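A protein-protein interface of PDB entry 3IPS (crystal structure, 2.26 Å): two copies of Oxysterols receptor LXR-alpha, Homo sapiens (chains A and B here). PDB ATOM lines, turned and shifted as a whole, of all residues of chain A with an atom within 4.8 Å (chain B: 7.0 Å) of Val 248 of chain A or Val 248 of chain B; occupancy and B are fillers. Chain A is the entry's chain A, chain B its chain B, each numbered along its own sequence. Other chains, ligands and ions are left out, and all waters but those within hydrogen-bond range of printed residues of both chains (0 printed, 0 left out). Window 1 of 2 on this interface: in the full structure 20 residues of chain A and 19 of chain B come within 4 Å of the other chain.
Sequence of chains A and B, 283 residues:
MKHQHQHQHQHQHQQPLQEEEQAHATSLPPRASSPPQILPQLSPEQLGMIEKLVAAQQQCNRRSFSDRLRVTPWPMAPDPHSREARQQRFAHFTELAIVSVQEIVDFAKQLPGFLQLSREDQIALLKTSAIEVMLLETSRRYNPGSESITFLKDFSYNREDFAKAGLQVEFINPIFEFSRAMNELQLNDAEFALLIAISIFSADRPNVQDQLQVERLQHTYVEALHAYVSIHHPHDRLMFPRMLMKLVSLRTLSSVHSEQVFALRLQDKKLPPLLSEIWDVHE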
ATOM      1  N   LEU A 244      20.123   5.549 -20.131  1.00  0.00           N
ATOM      2  CA  LEU A 244      19.580   6.813 -19.654  1.00  0.00           C
ATOM      3  C   LEU A 244      20.101   7.991 -20.466  1.00  0.00           C
ATOM      4  O   LEU A 244      19.321   8.803 -20.895  1.00  0.00           O
ATOM      5  CB  LEU A 244      19.914   7.030 -18.175  1.00  0.00           C
ATOM      6  CG  LEU A 244      19.120   6.228 -17.148  1.00  0.00           C
ATOM      7  CD1 LEU A 244      19.407   6.746 -15.747  1.00  0.00           C
ATOM      8  CD2 LEU A 244      17.611   6.280 -17.450  1.00  0.00           C
ATOM      9  N   MET A 245      21.410   8.092 -20.695  1.00  0.00           N
ATOM     10  CA  MET A 245      21.952   9.261 -21.387  1.00  0.00           C
ATOM     11  C   MET A 245      21.298   9.458 -22.765  1.00  0.00           C
ATOM     12  O   MET A 245      21.116  10.597 -23.200  1.00  0.00           O
ATOM     13  CB  MET A 245      23.470   9.182 -21.562  1.00  0.00           C
ATOM     14  CG  MET A 245      24.327   9.247 -20.301  1.00  0.00           C
ATOM     15  SD  MET A 245      24.176  10.734 -19.335  1.00  0.00           S
ATOM     16  CE  MET A 245      24.760  12.024 -20.442  1.00  0.00           C
ATOM     17  N   LYS A 246      20.946   8.364 -23.451  1.00  0.00           N
ATOM     18  CA  LYS A 246      20.191   8.440 -24.717  1.00  0.00           C
ATOM     19  C   LYS A 246      18.884   9.200 -24.585  1.00  0.00           C
ATOM     20  O   LYS A 246      18.344   9.664 -25.592  1.00  0.00           O
ATOM     21  CB  LYS A 246      19.879   7.044 -25.259  1.00  0.00           C
ATOM     22  CG  LYS A 246      21.094   6.290 -25.781  1.00  0.00           C
ATOM     23  CD  LYS A 246      21.404   6.649 -27.193  1.00  0.00           C
ATOM     24  CE  LYS A 246      22.827   6.286 -27.539  1.00  0.00           C
ATOM     25  NZ  LYS A 246      23.755   7.386 -27.151  1.00  0.00           N
ATOM     26  N   LEU A 247      18.359   9.324 -23.363  1.00  0.00           N
ATOM     27  CA  LEU A 247      17.188  10.175 -23.100  1.00  0.00           C
ATOM     28  C   LEU A 247      17.547  11.659 -23.223  1.00  0.00           C
ATOM     29  O   LEU A 247      16.717  12.464 -23.612  1.00  0.00           O
ATOM     30  CB  LEU A 247      16.556   9.868 -21.728  1.00  0.00           C
ATOM     31  CG  LEU A 247      15.352   8.912 -21.571  1.00  0.00           C
ATOM     32  CD1 LEU A 247      15.279   7.856 -22.654  1.00  0.00           C
ATOM     33  CD2 LEU A 247      15.377   8.279 -20.193  1.00  0.00           C
ATOM     34  N   VAL A 248      18.783  12.012 -22.888  1.00  0.00           N
ATOM     35  CA  VAL A 248      19.303  13.376 -23.129  1.00  0.00           C
ATOM     36  C   VAL A 248      19.229  13.797 -24.602  1.00  0.00           C
ATOM     37  O   VAL A 248      18.739  14.872 -24.901  1.00  0.00           O
ATOM     38  CB  VAL A 248      20.779  13.508 -22.692  1.00  0.00           C
ATOM     39  CG1 VAL A 248      21.318  14.946 -22.991  1.00  0.00           C
ATOM     40  CG2 VAL A 248      20.935  13.133 -21.223  1.00  0.00           C
ATOM     41  N   SER A 249      19.761  12.956 -25.499  1.00  0.00           N
ATOM     42  CA  SER A 249      19.694  13.151 -26.950  1.00  0.00           C
ATOM     43  C   SER A 249      18.259  13.293 -27.468  1.00  0.00           C
ATOM     44  O   SER A 249      17.983  14.179 -28.255  1.00  0.00           O
ATOM     45  CB  SER A 249      20.360  11.972 -27.683  1.00  0.00           C
ATOM     46  OG  SER A 249      21.646  11.660 -27.171  1.00  0.00           O
ATOM     47  N   LEU A 250      17.354  12.407 -27.049  1.00  0.00           N
ATOM     48  CA  LEU A 250      15.914  12.518 -27.396  1.00  0.00           C
ATOM     49  C   LEU A 250      15.264  13.897 -27.203  1.00  0.00           C
ATOM     50  O   LEU A 250      14.362  14.224 -27.943  1.00  0.00           O
ATOM     51  CB  LEU A 250      15.059  11.484 -26.641  1.00  0.00           C
ATOM     52  CG  LEU A 250      14.876  10.085 -27.239  1.00  0.00           C
ATOM     53  CD1 LEU A 250      14.003   9.238 -26.319  1.00  0.00           C
ATOM     54  CD2 LEU A 250      14.278  10.127 -28.615  1.00  0.00           C
ATOM     55  N   ARG A 251      15.673  14.669 -26.198  1.00  0.00           N
ATOM     56  CA  ARG A 251      15.119  16.017 -25.989  1.00  0.00           C
ATOM     57  C   ARG A 251      15.569  16.999 -27.036  1.00  0.00           C
ATOM     58  O   ARG A 251      14.883  18.000 -27.272  1.00  0.00           O
ATOM     59  CB  ARG A 251      15.580  16.611 -24.666  1.00  0.00           C
ATOM     60  CG  ARG A 251      14.930  16.068 -23.484  1.00  0.00           C
ATOM     61  CD  ARG A 251      13.437  16.289 -23.517  1.00  0.00           C
ATOM     62  NE  ARG A 251      12.924  15.627 -22.335  1.00  0.00           N
ATOM     63  CZ  ARG A 251      12.693  16.201 -21.154  1.00  0.00           C
ATOM     64  NH1 ARG A 251      12.805  17.510 -20.964  1.00  0.00           N
ATOM     65  NH2 ARG A 251      12.286  15.438 -20.168  1.00  0.00           N
ATOM     66  N   THR A 252      16.771  16.773 -27.581  1.00  0.00           N
ATOM     67  CA  THR A 252      17.277  17.583 -28.685  1.00  0.00           C
ATOM     68  C   THR A 252      16.531  17.206 -29.967  1.00  0.00           C
ATOM     69  O   THR A 252      16.141  18.088 -30.736  1.00  0.00           O
ATOM     70  CB  THR A 252      18.782  17.424 -28.872  1.00  0.00           C
ATOM     71  OG1 THR A 252      19.445  17.755 -27.641  1.00  0.00           O
ATOM     72  CG2 THR A 252      19.277  18.363 -29.970  1.00  0.00           C
ATOM     73  N   GLU B 132      24.217  25.225 -20.515  1.00  0.00           N
ATOM     74  CA  GLU B 132      23.816  24.191 -19.555  1.00  0.00           C
ATOM     75  C   GLU B 132      24.660  24.316 -18.274  1.00  0.00           C
ATOM     76  O   GLU B 132      24.185  24.013 -17.194  1.00  0.00           O
ATOM     77  CB  GLU B 132      23.998  22.780 -20.122  1.00  0.00           C
ATOM     78  CG  GLU B 132      23.239  22.441 -21.378  1.00  0.00           C
ATOM     79  CD  GLU B 132      23.366  20.960 -21.777  1.00  0.00           C
ATOM     80  OE1 GLU B 132      23.846  20.114 -20.975  1.00  0.00           O
ATOM     81  OE2 GLU B 132      22.981  20.639 -22.914  1.00  0.00           O
ATOM     82  N   SER B 202      29.736  15.782 -23.923  1.00  0.00           N
ATOM     83  CA  SER B 202      28.613  15.159 -24.638  1.00  0.00           C
ATOM     84  C   SER B 202      28.994  14.835 -26.071  1.00  0.00           C
ATOM     85  O   SER B 202      29.140  15.743 -26.883  1.00  0.00           O
ATOM     86  CB  SER B 202      27.389  16.089 -24.651  1.00  0.00           C
ATOM     87  OG  SER B 202      26.826  16.239 -23.343  1.00  0.00           O
ATOM     88  N   ASP B 204      27.331  14.013 -28.527  1.00  0.00           N
ATOM     89  CA  ASP B 204      26.325  14.274 -29.549  1.00  0.00           C
ATOM     90  C   ASP B 204      26.129  15.738 -29.954  1.00  0.00           C
ATOM     91  O   ASP B 204      25.340  16.017 -30.838  1.00  0.00           O
ATOM     92  CB  ASP B 204      24.985  13.607 -29.186  1.00  0.00           C
ATOM     93  CG  ASP B 204      24.305  14.214 -27.950  1.00  0.00           C
ATOM     94  OD1 ASP B 204      24.942  14.920 -27.144  1.00  0.00           O
ATOM     95  OD2 ASP B 204      23.100  13.953 -27.758  1.00  0.00           O
ATOM     96  N   ARG B 205      26.856  16.678 -29.354  1.00  0.00           N
ATOM     97  CA  ARG B 205      26.760  18.100 -29.768  1.00  0.00           C
ATOM     98  C   ARG B 205      26.968  18.281 -31.280  1.00  0.00           C
ATOM     99  O   ARG B 205      27.746  17.542 -31.897  1.00  0.00           O
ATOM    100  CB  ARG B 205      27.839  18.938 -29.089  1.00  0.00           C
ATOM    101  CG  ARG B 205      27.911  18.786 -27.619  1.00  0.00           C
ATOM    102  CD  ARG B 205      26.653  19.266 -26.984  1.00  0.00           C
ATOM    103  NE  ARG B 205      26.836  19.344 -25.554  1.00  0.00           N
ATOM    104  CZ  ARG B 205      25.884  19.637 -24.690  1.00  0.00           C
ATOM    105  NH1 ARG B 205      24.636  19.897 -25.107  1.00  0.00           N
ATOM    106  NH2 ARG B 205      26.185  19.639 -23.399  1.00  0.00           N
ATOM    107  N   GLN B 218      33.277  10.835 -21.237  1.00  0.00           N
ATOM    108  CA  GLN B 218      32.022  11.053 -20.503  1.00  0.00           C
ATOM    109  C   GLN B 218      31.693   9.908 -19.575  1.00  0.00           C
ATOM    110  O   GLN B 218      31.236  10.150 -18.454  1.00  0.00           O
ATOM    111  CB  GLN B 218      30.829  11.237 -21.433  1.00  0.00           C
ATOM    112  CG  GLN B 218      29.658  11.975 -20.748  1.00  0.00           C
ATOM    113  CD  GLN B 218      28.396  12.059 -21.592  1.00  0.00           C
ATOM    114  OE1 GLN B 218      27.998  11.078 -22.194  1.00  0.00           O
ATOM    115  NE2 GLN B 218      27.744  13.236 -21.618  1.00  0.00           N
ATOM    116  N   MET B 243      20.389  12.370 -10.678  1.00  0.00           N
ATOM    117  CA  MET B 243      21.322  13.415 -11.113  1.00  0.00           C
ATOM    118  C   MET B 243      21.572  13.431 -12.604  1.00  0.00           C
ATOM    119  O   MET B 243      21.801  14.501 -13.156  1.00  0.00           O
ATOM    120  CB  MET B 243      22.674  13.259 -10.429  1.00  0.00           C
ATOM    121  CG  MET B 243      22.688  13.769  -9.017  1.00  0.00           C
ATOM    122  SD  MET B 243      24.213  13.301  -8.265  1.00  0.00           S
ATOM    123  CE  MET B 243      23.611  13.024  -6.577  1.00  0.00           C
ATOM    124  N   LEU B 244      21.598  12.255 -13.238  1.00  0.00           N
ATOM    125  CA  LEU B 244      21.839  12.163 -14.686  1.00  0.00           C
ATOM    126  C   LEU B 244      20.625  12.666 -15.453  1.00  0.00           C
ATOM    127  O   LEU B 244      20.760  13.313 -16.473  1.00  0.00           O
ATOM    128  CB  LEU B 244      22.124  10.716 -15.122  1.00  0.00           C
ATOM    129  CG  LEU B 244      23.422  10.069 -14.681  1.00  0.00           C
ATOM    130  CD1 LEU B 244      23.532   8.704 -15.340  1.00  0.00           C
ATOM    131  CD2 LEU B 244      24.597  10.944 -15.048  1.00  0.00           C
ATOM    132  N   MET B 245      19.441  12.353 -14.938  1.00  0.00           N
ATOM    133  CA  MET B 245      18.173  12.784 -15.536  1.00  0.00           C
ATOM    134  C   MET B 245      18.051  14.309 -15.599  1.00  0.00           C
ATOM    135  O   MET B 245      17.246  14.850 -16.356  1.00  0.00           O
ATOM    136  CB  MET B 245      16.996  12.247 -14.731  1.00  0.00           C
ATOM    137  CG  MET B 245      16.915  10.715 -14.584  1.00  0.00           C
ATOM    138  SD  MET B 245      16.865   9.906 -16.160  1.00  0.00           S
ATOM    139  CE  MET B 245      15.350  10.485 -16.902  1.00  0.00           C
ATOM    140  N   LYS B 246      18.836  14.999 -14.794  1.00  0.00           N
ATOM    141  CA  LYS B 246      18.821  16.440 -14.823  1.00  0.00           C
ATOM    142  C   LYS B 246      19.486  16.963 -16.071  1.00  0.00           C
ATOM    143  O   LYS B 246      19.173  18.049 -16.485  1.00  0.00           O
ATOM    144  CB  LYS B 246      19.439  17.016 -13.539  1.00  0.00           C
ATOM    145  CG  LYS B 246      18.539  16.734 -12.266  1.00  0.00           C
ATOM    146  CD  LYS B 246      17.531  17.866 -11.937  1.00  0.00           C
ATOM    147  CE  LYS B 246      16.128  17.360 -11.584  1.00  0.00           C
ATOM    148  NZ  LYS B 246      15.161  17.598 -12.701  1.00  0.00           N
ATOM    149  N   LEU B 247      20.369  16.175 -16.689  1.00  0.00           N
ATOM    150  CA  LEU B 247      20.963  16.511 -17.969  1.00  0.00           C
ATOM    151  C   LEU B 247      19.926  16.462 -19.091  1.00  0.00           C
ATOM    152  O   LEU B 247      20.044  17.197 -20.069  1.00  0.00           O
ATOM    153  CB  LEU B 247      22.145  15.591 -18.307  1.00  0.00           C
ATOM    154  CG  LEU B 247      23.346  15.502 -17.340  1.00  0.00           C
ATOM    155  CD1 LEU B 247      24.143  14.217 -17.611  1.00  0.00           C
ATOM    156  CD2 LEU B 247      24.256  16.708 -17.417  1.00  0.00           C
ATOM    157  N   VAL B 248      18.904  15.621 -18.937  1.00  0.00           N
ATOM    158  CA  VAL B 248      17.745  15.622 -19.849  1.00  0.00           C
ATOM    159  C   VAL B 248      17.052  16.978 -19.812  1.00  0.00           C
ATOM    160  O   VAL B 248      16.947  17.632 -20.821  1.00  0.00           O
ATOM    161  CB  VAL B 248      16.748  14.514 -19.506  1.00  0.00           C
ATOM    162  CG1 VAL B 248      15.539  14.588 -20.422  1.00  0.00           C
ATOM    163  CG2 VAL B 248      17.418  13.148 -19.621  1.00  0.00           C
ATOM    164  N   SER B 249      16.637  17.426 -18.625  1.00  0.00           N
ATOM    165  CA  SER B 249      15.988  18.740 -18.470  1.00  0.00           C
ATOM    166  C   SER B 249      16.820  19.887 -19.017  1.00  0.00           C
ATOM    167  O   SER B 249      16.267  20.828 -19.539  1.00  0.00           O
ATOM    168  CB  SER B 249      15.690  19.029 -16.998  1.00  0.00           C
ATOM    169  OG  SER B 249      14.743  18.110 -16.462  1.00  0.00           O
ATOM    170  N   LEU B 250      18.142  19.819 -18.872  1.00  0.00           N
ATOM    171  CA  LEU B 250      19.041  20.881 -19.356  1.00  0.00           C
ATOM    172  C   LEU B 250      19.106  20.967 -20.886  1.00  0.00           C
ATOM    173  O   LEU B 250      19.370  22.022 -21.425  1.00  0.00           O
ATOM    174  CB  LEU B 250      20.464  20.695 -18.801  1.00  0.00           C
ATOM    175  CG  LEU B 250      20.889  21.378 -17.502  1.00  0.00           C
ATOM    176  CD1 LEU B 250      22.357  21.013 -17.208  1.00  0.00           C
ATOM    177  CD2 LEU B 250      20.749  22.876 -17.571  1.00  0.00           C
ATOM    178  N   ARG B 251      18.883  19.874 -21.597  1.00  0.00           N
ATOM    179  CA  ARG B 251      18.781  19.949 -23.064  1.00  0.00           C
ATOM    180  C   ARG B 251      17.589  20.760 -23.448  1.00  0.00           C
ATOM    181  O   ARG B 251      17.704  21.611 -24.311  1.00  0.00           O
ATOM    182  CB  ARG B 251      18.622  18.586 -23.732  1.00  0.00           C
ATOM    183  CG  ARG B 251      19.862  17.813 -23.882  1.00  0.00           C
ATOM    184  CD  ARG B 251      20.943  18.467 -24.726  1.00  0.00           C
ATOM    185  NE  ARG B 251      22.150  17.673 -24.528  1.00  0.00           N
ATOM    186  CZ  ARG B 251      22.639  16.787 -25.387  1.00  0.00           C
ATOM    187  NH1 ARG B 251      22.101  16.604 -26.588  1.00  0.00           N
ATOM    188  NH2 ARG B 251      23.718  16.102 -25.050  1.00  0.00           N
ATOM    189  N   THR B 252      16.441  20.482 -22.832  1.00  0.00           N
ATOM    190  CA  THR B 252      15.225  21.287 -23.046  1.00  0.00           C
ATOM    191  C   THR B 252      15.474  22.775 -22.777  1.00  0.00           C
ATOM    192  O   THR B 252      15.128  23.617 -23.589  1.00  0.00           O
ATOM    193  CB  THR B 252      14.048  20.793 -22.177  1.00  0.00           C
ATOM    194  OG1 THR B 252      13.454  19.643 -22.788  1.00  0.00           O
ATOM    195  CG2 THR B 252      12.996  21.852 -22.063  1.00  0.00           C
ATOM    196  N   LEU B 253      16.103  23.093 -21.652  1.00  0.00           N
ATOM    197  CA  LEU B 253      16.409  24.502 -21.314  1.00  0.00           C
ATOM    198  C   LEU B 253      17.333  25.147 -22.347  1.00  0.00           C
ATOM    199  O   LEU B 253      17.175  26.322 -22.724  1.00  0.00           O
ATOM    200  CB  LEU B 253      17.046  24.593 -19.922  1.00  0.00           C
ATOM    201  CG  LEU B 253      16.127  24.243 -18.754  1.00  0.00           C
ATOM    202  CD1 LEU B 253      16.884  24.139 -17.474  1.00  0.00           C
ATOM    203  CD2 LEU B 253      15.087  25.308 -18.646  1.00  0.00           C
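Among the printed residues, pairs that only touch across the chains: Leu 244 of chain A with Met 245 of chain B (3.9 Å), Met 245 of chain A with Gln 218 of chain B (3.4 Å), Met 245 of chain A with Leu 247 of chain B (3.6 Å), Leu 247 of chain A with Met 245 of chain B (3.96 Å), Leu 247 of chain A with Val 248 of chain B (3.9 Å), Val 248 of chain A with Leu 247 of chain B (3.9 Å), Val 248 of chain A with Val 248 of chain B (3.7 Å), Val 248 of chain A with Arg 251 of chain B (3.2 Å), Arg 251 of chain A with Val 248 of chain B (3.4 Å) and Arg 251 of chain A with Arg 251 of chain B (3.7 Å).
Of the 16 printed residues of chain B, 7 touch a printed residue of chain A.
Printed residues of chain B that touch a printed residue of chain A: Asp 204, Gln 218, Met 245, Leu 247, Val 248, Arg 251 and Thr 252.
Hydrophobic or aromatic side chains of chain B that line the printed part of chain A: Met 245, Leu 247 and Val 248.
Along chain B the printed residues that touch a printed residue of chain A span positions 204 to 252.
Of the 9 printed residues of chain A, 7 touch a printed residue of chain B.
Hydrophobic or aromatic side chains of chain A within 4 Å of the printed part of chain B: Leu 244, Met 245, Leu 247 and Val 248.
Along chain A the printed residues that touch a printed residue of chain B span positions 244 to 252.
The guanidinium group (NH2) of Arg 251 of chain B lies within salt-bridge range of the side-chain carboxylate (OD1) of Asp 204 of chain B, 2.7 Å away.
The guanidinium group (NE) of Arg 251 of chain B is in salt-bridge range of the side-chain carboxylate (OE2) of Glu 132 of chain B (3.5 Å).
The side-chain hydroxyl (OG) of Ser 249 of chain A sits at hydrogen-bond distance from the side-chain carboxylate (OD2) of Asp 204 of chain B.
OG1 of Thr 252 of chain B lies within hydrogen-bond range of NH1 of Arg 251 of chain A (2.9 Å).
The side-chain hydroxyl of Thr 252 of chain A sits at hydrogen-bond distance from the guanidinium group of Arg 251 of chain B (3.1 Å).
Leu 244 of chain A touches Met 245 of chain B, but with the chains exchanged Met 245 of chain A does not touch Leu 244 of chain B (4.3 Å).
Met 245 of chain A touches Leu 247 of chain B, and with the chains exchanged Leu 247 of chain A touches Met 245 of chain B.
Val 248 of chain A touches its own counterpart, Val 248 of chain B.
Val 248 of chain A touches Arg 251 of chain B, and with the chains exchanged Arg 251 of chain A touches Val 248 of chain B.
Positions printed for both chains: 244, 245, 246, 247, 248, 249, 250, 251 and 252.
Of the 13 pairs that touch across the chains among the printed residues, 10 have their exchanged pair printed and touching as well.
Of chain B, only Leu 247 (3.9 Å), Val 248 (3.7 Å) and Arg 251 (3.2 Å) come within 4 Å of Val 248 of chain A.
Val 248 of chain B touches just these residues of chain A: Leu 247, Val 248 and Arg 251.
Printed residues of chain B within 4 Å of Met 245 of chain A: Gln 218 (3.4 Å) and Leu 247 (3.6 Å).
Of the printed residues of chain A, Asp 204 of chain B touches Ser 249.
Of the printed residues of chain B, Thr 252 of chain A touches Arg 251.
Leu 253 of chain B touches none of the printed residues of chain A.
The nearest printed residue of chain A that does not touch Val 248 of chain B is Leu 244 of chain A (4.9 Å).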
